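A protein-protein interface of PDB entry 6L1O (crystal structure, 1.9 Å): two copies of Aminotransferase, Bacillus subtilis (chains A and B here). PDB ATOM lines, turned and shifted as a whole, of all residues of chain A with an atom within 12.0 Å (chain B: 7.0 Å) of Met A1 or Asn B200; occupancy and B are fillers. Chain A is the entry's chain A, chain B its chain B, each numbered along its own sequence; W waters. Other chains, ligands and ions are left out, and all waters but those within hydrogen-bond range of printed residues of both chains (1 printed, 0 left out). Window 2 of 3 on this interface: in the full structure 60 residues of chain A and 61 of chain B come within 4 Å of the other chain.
N of Thr A4 sits at hydrogen-bond distance from NE2 of His B202 (3.1 Å).
The backbone carbonyl oxygen (O) of Lys B169 sits at hydrogen-bond distance from a ring nitrogen (ND1) of His B202, at 2.8 Å.
Among the printed residues, pairs that only touch across the chains: Met A1 with Asn B200 (3.1 Å), Met A1 with Thr B229 (3.95 Å), Ile A3 with His B202 (3.8 Å), Ile A3 with Thr B229 (3.7 Å) and Ile A3 with Asn B254 (3.4 Å).
Of the printed residues of chain B, Ile A3 touches His B202, Thr B229 and Asn B254. Of the printed residues of chain B, Thr A4 touches His B202 (3.1 Å). Ser A6 touches none of the printed residues of chain B. No residue of chain A comes within 4 Å of Ala B168. No residue of chain A comes within 4 Å of Lys B169. Leu B170 touches none of the printed residues of chain A. No residue of chain A comes within 4 Å of Glu B198. His B199 touches none of the printed residues of chain A. Thr B229 touches just these residues of chain A: Met A1 and Ile A3. No residue of chain A comes within 4 Å of Val B230. Printed residues of chain A within 4 Å of Asn B254: Ile A3. The nearest printed residue of chain B that does not touch Met A1 is Lys B197 (4.002 Å).
Printed residues of chain A that touch a printed residue of chain B: Met A1, Ile A3 and Thr A4. Hydrophobic or aromatic side chains of chain A that line the printed part of chain B: Met A1 and Ile A3. Along chain A the printed residues that touch a printed residue of chain B span positions 1 to 4. Among the printed residues, 6 pairs touch across the chains. Among the printed residues, no Asp or Glu carboxylate lies within 4 Å of a Lys or Arg side-chain nitrogen of the other chain.
No position is printed for both chains. Of the 6 pairs that touch across the chains among the printed residues, none has its exchanged pair printed and touching as well.
Water W1 bridges the backbone carbonyl oxygen of Met A1 and the backbone carbonyl oxygen of Thr B229.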
ATOM      1  N   MET A   1      30.257  20.581 -20.708  1.00  0.00           N
ATOM      2  CA  MET A   1      31.158  21.786 -20.627  1.00  0.00           C
ATOM      3  C   MET A   1      31.117  22.339 -19.194  1.00  0.00           C
ATOM      4  O   MET A   1      31.793  21.814 -18.311  1.00  0.00           O
ATOM      5  CB  MET A   1      30.738  22.841 -21.661  1.00  0.00           C
ATOM      6  N   GLU A   2      30.313  23.364 -18.942  1.00  0.00           N
ATOM      7  CA  GLU A   2      30.134  23.846 -17.576  1.00  0.00           C
ATOM      8  C   GLU A   2      28.811  23.328 -16.976  1.00  0.00           C
ATOM      9  O   GLU A   2      27.726  23.611 -17.464  1.00  0.00           O
ATOM     10  CB  GLU A   2      30.198  25.366 -17.487  1.00  0.00           C
ATOM     11  CG  GLU A   2      30.184  25.868 -16.037  1.00  0.00           C
ATOM     12  CD  GLU A   2      31.093  27.064 -15.789  1.00  0.00           C
ATOM     13  OE1 GLU A   2      31.351  27.825 -16.747  1.00  0.00           O
ATOM     14  OE2 GLU A   2      31.547  27.253 -14.626  1.00  0.00           O
ATOM     15  N   ILE A   3      28.938  22.568 -15.903  1.00  0.00           N
ATOM     16  CA  ILE A   3      27.791  22.069 -15.159  1.00  0.00           C
ATOM     17  C   ILE A   3      27.232  23.213 -14.289  1.00  0.00           C
ATOM     18  O   ILE A   3      27.971  23.868 -13.572  1.00  0.00           O
ATOM     19  CB  ILE A   3      28.176  20.853 -14.306  1.00  0.00           C
ATOM     20  CG1 ILE A   3      28.768  19.738 -15.206  1.00  0.00           C
ATOM     21  CG2 ILE A   3      26.966  20.354 -13.495  1.00  0.00           C
ATOM     22  CD1 ILE A   3      27.809  19.121 -16.215  1.00  0.00           C
ATOM     23  N   THR A   4      25.928  23.443 -14.407  1.00  0.00           N
ATOM     24  CA  THR A   4      25.213  24.504 -13.746  1.00  0.00           C
ATOM     25  C   THR A   4      24.072  24.001 -12.780  1.00  0.00           C
ATOM     26  O   THR A   4      22.936  23.810 -13.201  1.00  0.00           O
ATOM     27  CB  THR A   4      24.617  25.453 -14.810  1.00  0.00           C
ATOM     28  OG1 THR A   4      25.669  25.901 -15.691  1.00  0.00           O
ATOM     29  CG2 THR A   4      23.944  26.661 -14.135  1.00  0.00           C
ATOM     30  N   PRO A   5      24.386  23.818 -11.487  1.00  0.00           N
ATOM     31  CA  PRO A   5      23.320  23.587 -10.505  1.00  0.00           C
ATOM     32  C   PRO A   5      22.232  24.663 -10.539  1.00  0.00           C
ATOM     33  O   PRO A   5      22.496  25.814 -10.870  1.00  0.00           O
ATOM     34  CB  PRO A   5      24.063  23.598  -9.155  1.00  0.00           C
ATOM     35  CG  PRO A   5      25.467  23.304  -9.490  1.00  0.00           C
ATOM     36  CD  PRO A   5      25.724  23.838 -10.866  1.00  0.00           C
ATOM     37  N   SER A   6      21.009  24.288 -10.200  1.00  0.00           N
ATOM     38  CA  SER A   6      19.921  25.237 -10.123  1.00  0.00           C
ATOM     39  C   SER A   6      20.082  26.217  -8.935  1.00  0.00           C
ATOM     40  O   SER A   6      20.932  26.049  -8.063  1.00  0.00           O
ATOM     41  CB  SER A   6      18.594  24.482  -9.962  1.00  0.00           C
ATOM     42  OG  SER A   6      18.501  23.982  -8.643  1.00  0.00           O
ATOM     43  N   LEU B 165      18.122  26.168 -28.079  1.00  0.00           N
ATOM     44  CA  LEU B 165      19.301  25.517 -27.539  1.00  0.00           C
ATOM     45  C   LEU B 165      20.000  26.394 -26.522  1.00  0.00           C
ATOM     46  O   LEU B 165      20.807  25.903 -25.754  1.00  0.00           O
ATOM     47  CB  LEU B 165      20.270  25.098 -28.644  1.00  0.00           C
ATOM     48  CG  LEU B 165      19.704  24.073 -29.630  1.00  0.00           C
ATOM     49  CD1 LEU B 165      20.716  23.721 -30.699  1.00  0.00           C
ATOM     50  CD2 LEU B 165      19.271  22.803 -28.916  1.00  0.00           C
ATOM     51  N   GLU B 166      19.715  27.697 -26.532  1.00  0.00           N
ATOM     52  CA  GLU B 166      20.281  28.596 -25.548  1.00  0.00           C
ATOM     53  C   GLU B 166      19.661  28.358 -24.193  1.00  0.00           C
ATOM     54  O   GLU B 166      20.373  28.207 -23.215  1.00  0.00           O
ATOM     55  CB  GLU B 166      20.064  30.051 -25.970  1.00  0.00           C
ATOM     56  CG  GLU B 166      20.676  31.086 -25.017  1.00  0.00           C
ATOM     57  CD  GLU B 166      22.200  31.004 -24.899  1.00  0.00           C
ATOM     58  OE1 GLU B 166      22.864  30.413 -25.792  1.00  0.00           O
ATOM     59  OE2 GLU B 166      22.746  31.542 -23.903  1.00  0.00           O
ATOM     60  N   LYS B 167      18.334  28.303 -24.161  1.00  0.00           N
ATOM     61  CA  LYS B 167      17.604  28.176 -22.904  1.00  0.00           C
ATOM     62  C   LYS B 167      17.520  26.715 -22.429  1.00  0.00           C
ATOM     63  O   LYS B 167      17.197  26.438 -21.268  1.00  0.00           O
ATOM     64  CB  LYS B 167      16.213  28.805 -23.034  1.00  0.00           C
ATOM     65  CG  LYS B 167      15.900  29.805 -21.921  1.00  0.00           C
ATOM     66  CD  LYS B 167      14.991  30.952 -22.387  1.00  0.00           C
ATOM     67  CE  LYS B 167      13.538  30.512 -22.543  1.00  0.00           C
ATOM     68  NZ  LYS B 167      12.619  31.667 -22.749  1.00  0.00           N
ATOM     69  N   ALA B 168      17.822  25.776 -23.331  1.00  0.00           N
ATOM     70  CA  ALA B 168      17.759  24.338 -22.985  1.00  0.00           C
ATOM     71  C   ALA B 168      18.838  23.925 -21.980  1.00  0.00           C
ATOM     72  O   ALA B 168      20.000  23.991 -22.278  1.00  0.00           O
ATOM     73  CB  ALA B 168      17.841  23.494 -24.242  1.00  0.00           C
ATOM     74  N   LYS B 169      18.425  23.500 -20.771  1.00  0.00           N
ATOM     75  CA  LYS B 169      19.354  23.078 -19.740  1.00  0.00           C
ATOM     76  C   LYS B 169      19.365  21.583 -19.492  1.00  0.00           C
ATOM     77  O   LYS B 169      20.310  21.064 -18.955  1.00  0.00           O
ATOM     78  CB  LYS B 169      19.128  23.844 -18.425  1.00  0.00           C
ATOM     79  CG  LYS B 169      19.300  25.363 -18.521  1.00  0.00           C
ATOM     80  CD  LYS B 169      20.628  25.780 -19.147  1.00  0.00           C
ATOM     81  CE  LYS B 169      20.647  27.270 -19.483  1.00  0.00           C
ATOM     82  NZ  LYS B 169      21.833  27.630 -20.339  1.00  0.00           N
ATOM     83  N   LEU B 170      18.336  20.887 -19.928  1.00  0.00           N
ATOM     84  CA  LEU B 170      18.198  19.476 -19.579  1.00  0.00           C
ATOM     85  C   LEU B 170      17.621  18.705 -20.753  1.00  0.00           C
ATOM     86  O   LEU B 170      16.793  19.223 -21.468  1.00  0.00           O
ATOM     87  CB  LEU B 170      17.275  19.336 -18.401  1.00  0.00           C
ATOM     88  CG  LEU B 170      17.015  17.872 -17.970  1.00  0.00           C
ATOM     89  CD1 LEU B 170      18.129  17.425 -17.068  1.00  0.00           C
ATOM     90  CD2 LEU B 170      15.690  17.689 -17.271  1.00  0.00           C
ATOM     91  N   PHE B 195      26.424  16.574 -28.885  1.00  0.00           N
ATOM     92  CA  PHE B 195      25.415  17.580 -29.005  1.00  0.00           C
ATOM     93  C   PHE B 195      25.217  18.339 -27.695  1.00  0.00           C
ATOM     94  O   PHE B 195      25.111  19.579 -27.704  1.00  0.00           O
ATOM     95  CB  PHE B 195      24.092  16.990 -29.465  1.00  0.00           C
ATOM     96  CG  PHE B 195      23.058  18.019 -29.805  1.00  0.00           C
ATOM     97  CD1 PHE B 195      23.035  18.612 -31.070  1.00  0.00           C
ATOM     98  CD2 PHE B 195      22.063  18.355 -28.904  1.00  0.00           C
ATOM     99  CE1 PHE B 195      22.050  19.543 -31.402  1.00  0.00           C
ATOM    100  CE2 PHE B 195      21.068  19.275 -29.223  1.00  0.00           C
ATOM    101  CZ  PHE B 195      21.073  19.885 -30.482  1.00  0.00           C
ATOM    102  N   ALA B 196      25.139  17.612 -26.578  1.00  0.00           N
ATOM    103  CA  ALA B 196      24.919  18.261 -25.279  1.00  0.00           C
ATOM    104  C   ALA B 196      26.074  19.157 -24.893  1.00  0.00           C
ATOM    105  O   ALA B 196      25.879  20.252 -24.341  1.00  0.00           O
ATOM    106  CB  ALA B 196      24.682  17.223 -24.209  1.00  0.00           C
ATOM    107  N   LYS B 197      27.269  18.663 -25.167  1.00  0.00           N
ATOM    108  CA  LYS B 197      28.512  19.368 -24.844  1.00  0.00           C
ATOM    109  C   LYS B 197      28.562  20.707 -25.594  1.00  0.00           C
ATOM    110  O   LYS B 197      28.859  21.734 -25.016  1.00  0.00           O
ATOM    111  CB  LYS B 197      29.719  18.498 -25.190  1.00  0.00           C
ATOM    112  CG  LYS B 197      31.047  19.088 -24.699  1.00  0.00           C
ATOM    113  CD  LYS B 197      32.223  18.202 -25.069  1.00  0.00           C
ATOM    114  CE  LYS B 197      33.408  18.408 -24.130  1.00  0.00           C
ATOM    115  NZ  LYS B 197      34.562  19.033 -24.831  1.00  0.00           N
ATOM    116  N   GLU B 198      28.192  20.671 -26.859  1.00  0.00           N
ATOM    117  CA  GLU B 198      28.197  21.843 -27.739  1.00  0.00           C
ATOM    118  C   GLU B 198      27.217  22.937 -27.308  1.00  0.00           C
ATOM    119  O   GLU B 198      27.501  24.145 -27.429  1.00  0.00           O
ATOM    120  CB  GLU B 198      27.856  21.395 -29.179  1.00  0.00           C
ATOM    121  CG  GLU B 198      27.940  22.511 -30.226  1.00  0.00           C
ATOM    122  CD  GLU B 198      29.356  23.085 -30.331  1.00  0.00           C
ATOM    123  OE1 GLU B 198      30.313  22.284 -30.384  1.00  0.00           O
ATOM    124  OE2 GLU B 198      29.528  24.327 -30.311  1.00  0.00           O
ATOM    125  N   HIS B 199      26.063  22.543 -26.797  1.00  0.00           N
ATOM    126  CA  HIS B 199      25.035  23.536 -26.433  1.00  0.00           C
ATOM    127  C   HIS B 199      24.789  23.654 -24.917  1.00  0.00           C
ATOM    128  O   HIS B 199      23.801  24.250 -24.496  1.00  0.00           O
ATOM    129  CB  HIS B 199      23.753  23.226 -27.168  1.00  0.00           C
ATOM    130  CG  HIS B 199      23.903  23.237 -28.656  1.00  0.00           C
ATOM    131  ND1 HIS B 199      24.019  24.404 -29.390  1.00  0.00           N
ATOM    132  CD2 HIS B 199      23.965  22.224 -29.549  1.00  0.00           C
ATOM    133  CE1 HIS B 199      24.135  24.104 -30.671  1.00  0.00           C
ATOM    134  NE2 HIS B 199      24.108  22.789 -30.794  1.00  0.00           N
ATOM    135  N   ASN B 200      25.665  23.034 -24.126  1.00  0.00           N
ATOM    136  CA  ASN B 200      25.614  23.098 -22.661  1.00  0.00           C
ATOM    137  C   ASN B 200      24.284  22.611 -22.117  1.00  0.00           C
ATOM    138  O   ASN B 200      23.546  23.349 -21.467  1.00  0.00           O
ATOM    139  CB  ASN B 200      25.884  24.530 -22.156  1.00  0.00           C
ATOM    140  CG  ASN B 200      27.179  25.058 -22.687  1.00  0.00           C
ATOM    141  OD1 ASN B 200      28.241  24.519 -22.371  1.00  0.00           O
ATOM    142  ND2 ASN B 200      27.108  26.067 -23.566  1.00  0.00           N
ATOM    143  N   ILE B 201      23.968  21.369 -22.449  1.00  0.00           N
ATOM    144  CA  ILE B 201      22.743  20.726 -21.981  1.00  0.00           C
ATOM    145  C   ILE B 201      23.177  19.605 -21.057  1.00  0.00           C
ATOM    146  O   ILE B 201      24.020  18.810 -21.428  1.00  0.00           O
ATOM    147  CB  ILE B 201      21.929  20.185 -23.148  1.00  0.00           C
ATOM    148  CG1 ILE B 201      21.638  21.304 -24.165  1.00  0.00           C
ATOM    149  CG2 ILE B 201      20.637  19.539 -22.637  1.00  0.00           C
ATOM    150  CD1 ILE B 201      21.081  20.811 -25.500  1.00  0.00           C
ATOM    151  N   HIS B 202      22.612  19.564 -19.846  1.00  0.00           N
ATOM    152  CA  HIS B 202      22.779  18.424 -18.978  1.00  0.00           C
ATOM    153  C   HIS B 202      21.941  17.229 -19.544  1.00  0.00           C
ATOM    154  O   HIS B 202      20.758  17.344 -19.752  1.00  0.00           O
ATOM    155  CB  HIS B 202      22.288  18.721 -17.573  1.00  0.00           C
ATOM    156  CG  HIS B 202      22.932  19.923 -16.948  1.00  0.00           C
ATOM    157  ND1 HIS B 202      22.413  21.188 -17.072  1.00  0.00           N
ATOM    158  CD2 HIS B 202      24.040  20.045 -16.194  1.00  0.00           C
ATOM    159  CE1 HIS B 202      23.162  22.046 -16.401  1.00  0.00           C
ATOM    160  NE2 HIS B 202      24.149  21.374 -15.852  1.00  0.00           N
ATOM    161  N   THR B 229      31.002  13.947 -19.013  1.00  0.00           N
ATOM    162  CA  THR B 229      31.258  15.379 -19.077  1.00  0.00           C
ATOM    163  C   THR B 229      29.979  16.178 -19.039  1.00  0.00           C
ATOM    164  O   THR B 229      29.963  17.294 -18.534  1.00  0.00           O
ATOM    165  CB  THR B 229      32.021  15.750 -20.383  1.00  0.00           C
ATOM    166  OG1 THR B 229      33.231  15.006 -20.437  1.00  0.00           O
ATOM    167  CG2 THR B 229      32.330  17.227 -20.451  1.00  0.00           C
ATOM    168  N   VAL B 230      28.907  15.616 -19.590  1.00  0.00           N
ATOM    169  CA  VAL B 230      27.688  16.359 -19.797  1.00  0.00           C
ATOM    170  C   VAL B 230      26.509  15.850 -18.947  1.00  0.00           C
ATOM    171  O   VAL B 230      25.474  16.466 -18.903  1.00  0.00           O
ATOM    172  CB  VAL B 230      27.258  16.354 -21.282  1.00  0.00           C
ATOM    173  CG1 VAL B 230      28.321  16.979 -22.159  1.00  0.00           C
ATOM    174  CG2 VAL B 230      26.941  14.958 -21.779  1.00  0.00           C
ATOM    175  N   ASN B 254      28.495  12.507 -13.962  1.00  0.00           N
ATOM    176  CA  ASN B 254      29.255  13.697 -13.739  1.00  0.00           C
ATOM    177  C   ASN B 254      29.276  14.096 -12.267  1.00  0.00           C
ATOM    178  O   ASN B 254      28.215  14.247 -11.622  1.00  0.00           O
ATOM    179  CB  ASN B 254      28.653  14.823 -14.548  1.00  0.00           C
ATOM    180  CG  ASN B 254      29.427  16.097 -14.368  1.00  0.00           C
ATOM    181  OD1 ASN B 254      29.145  16.852 -13.447  1.00  0.00           O
ATOM    182  ND2 ASN B 254      30.477  16.288 -15.168  1.00  0.00           N
HETATM  183  O   HOH W   1      31.537  19.387 -17.639  1.00  0.00           O
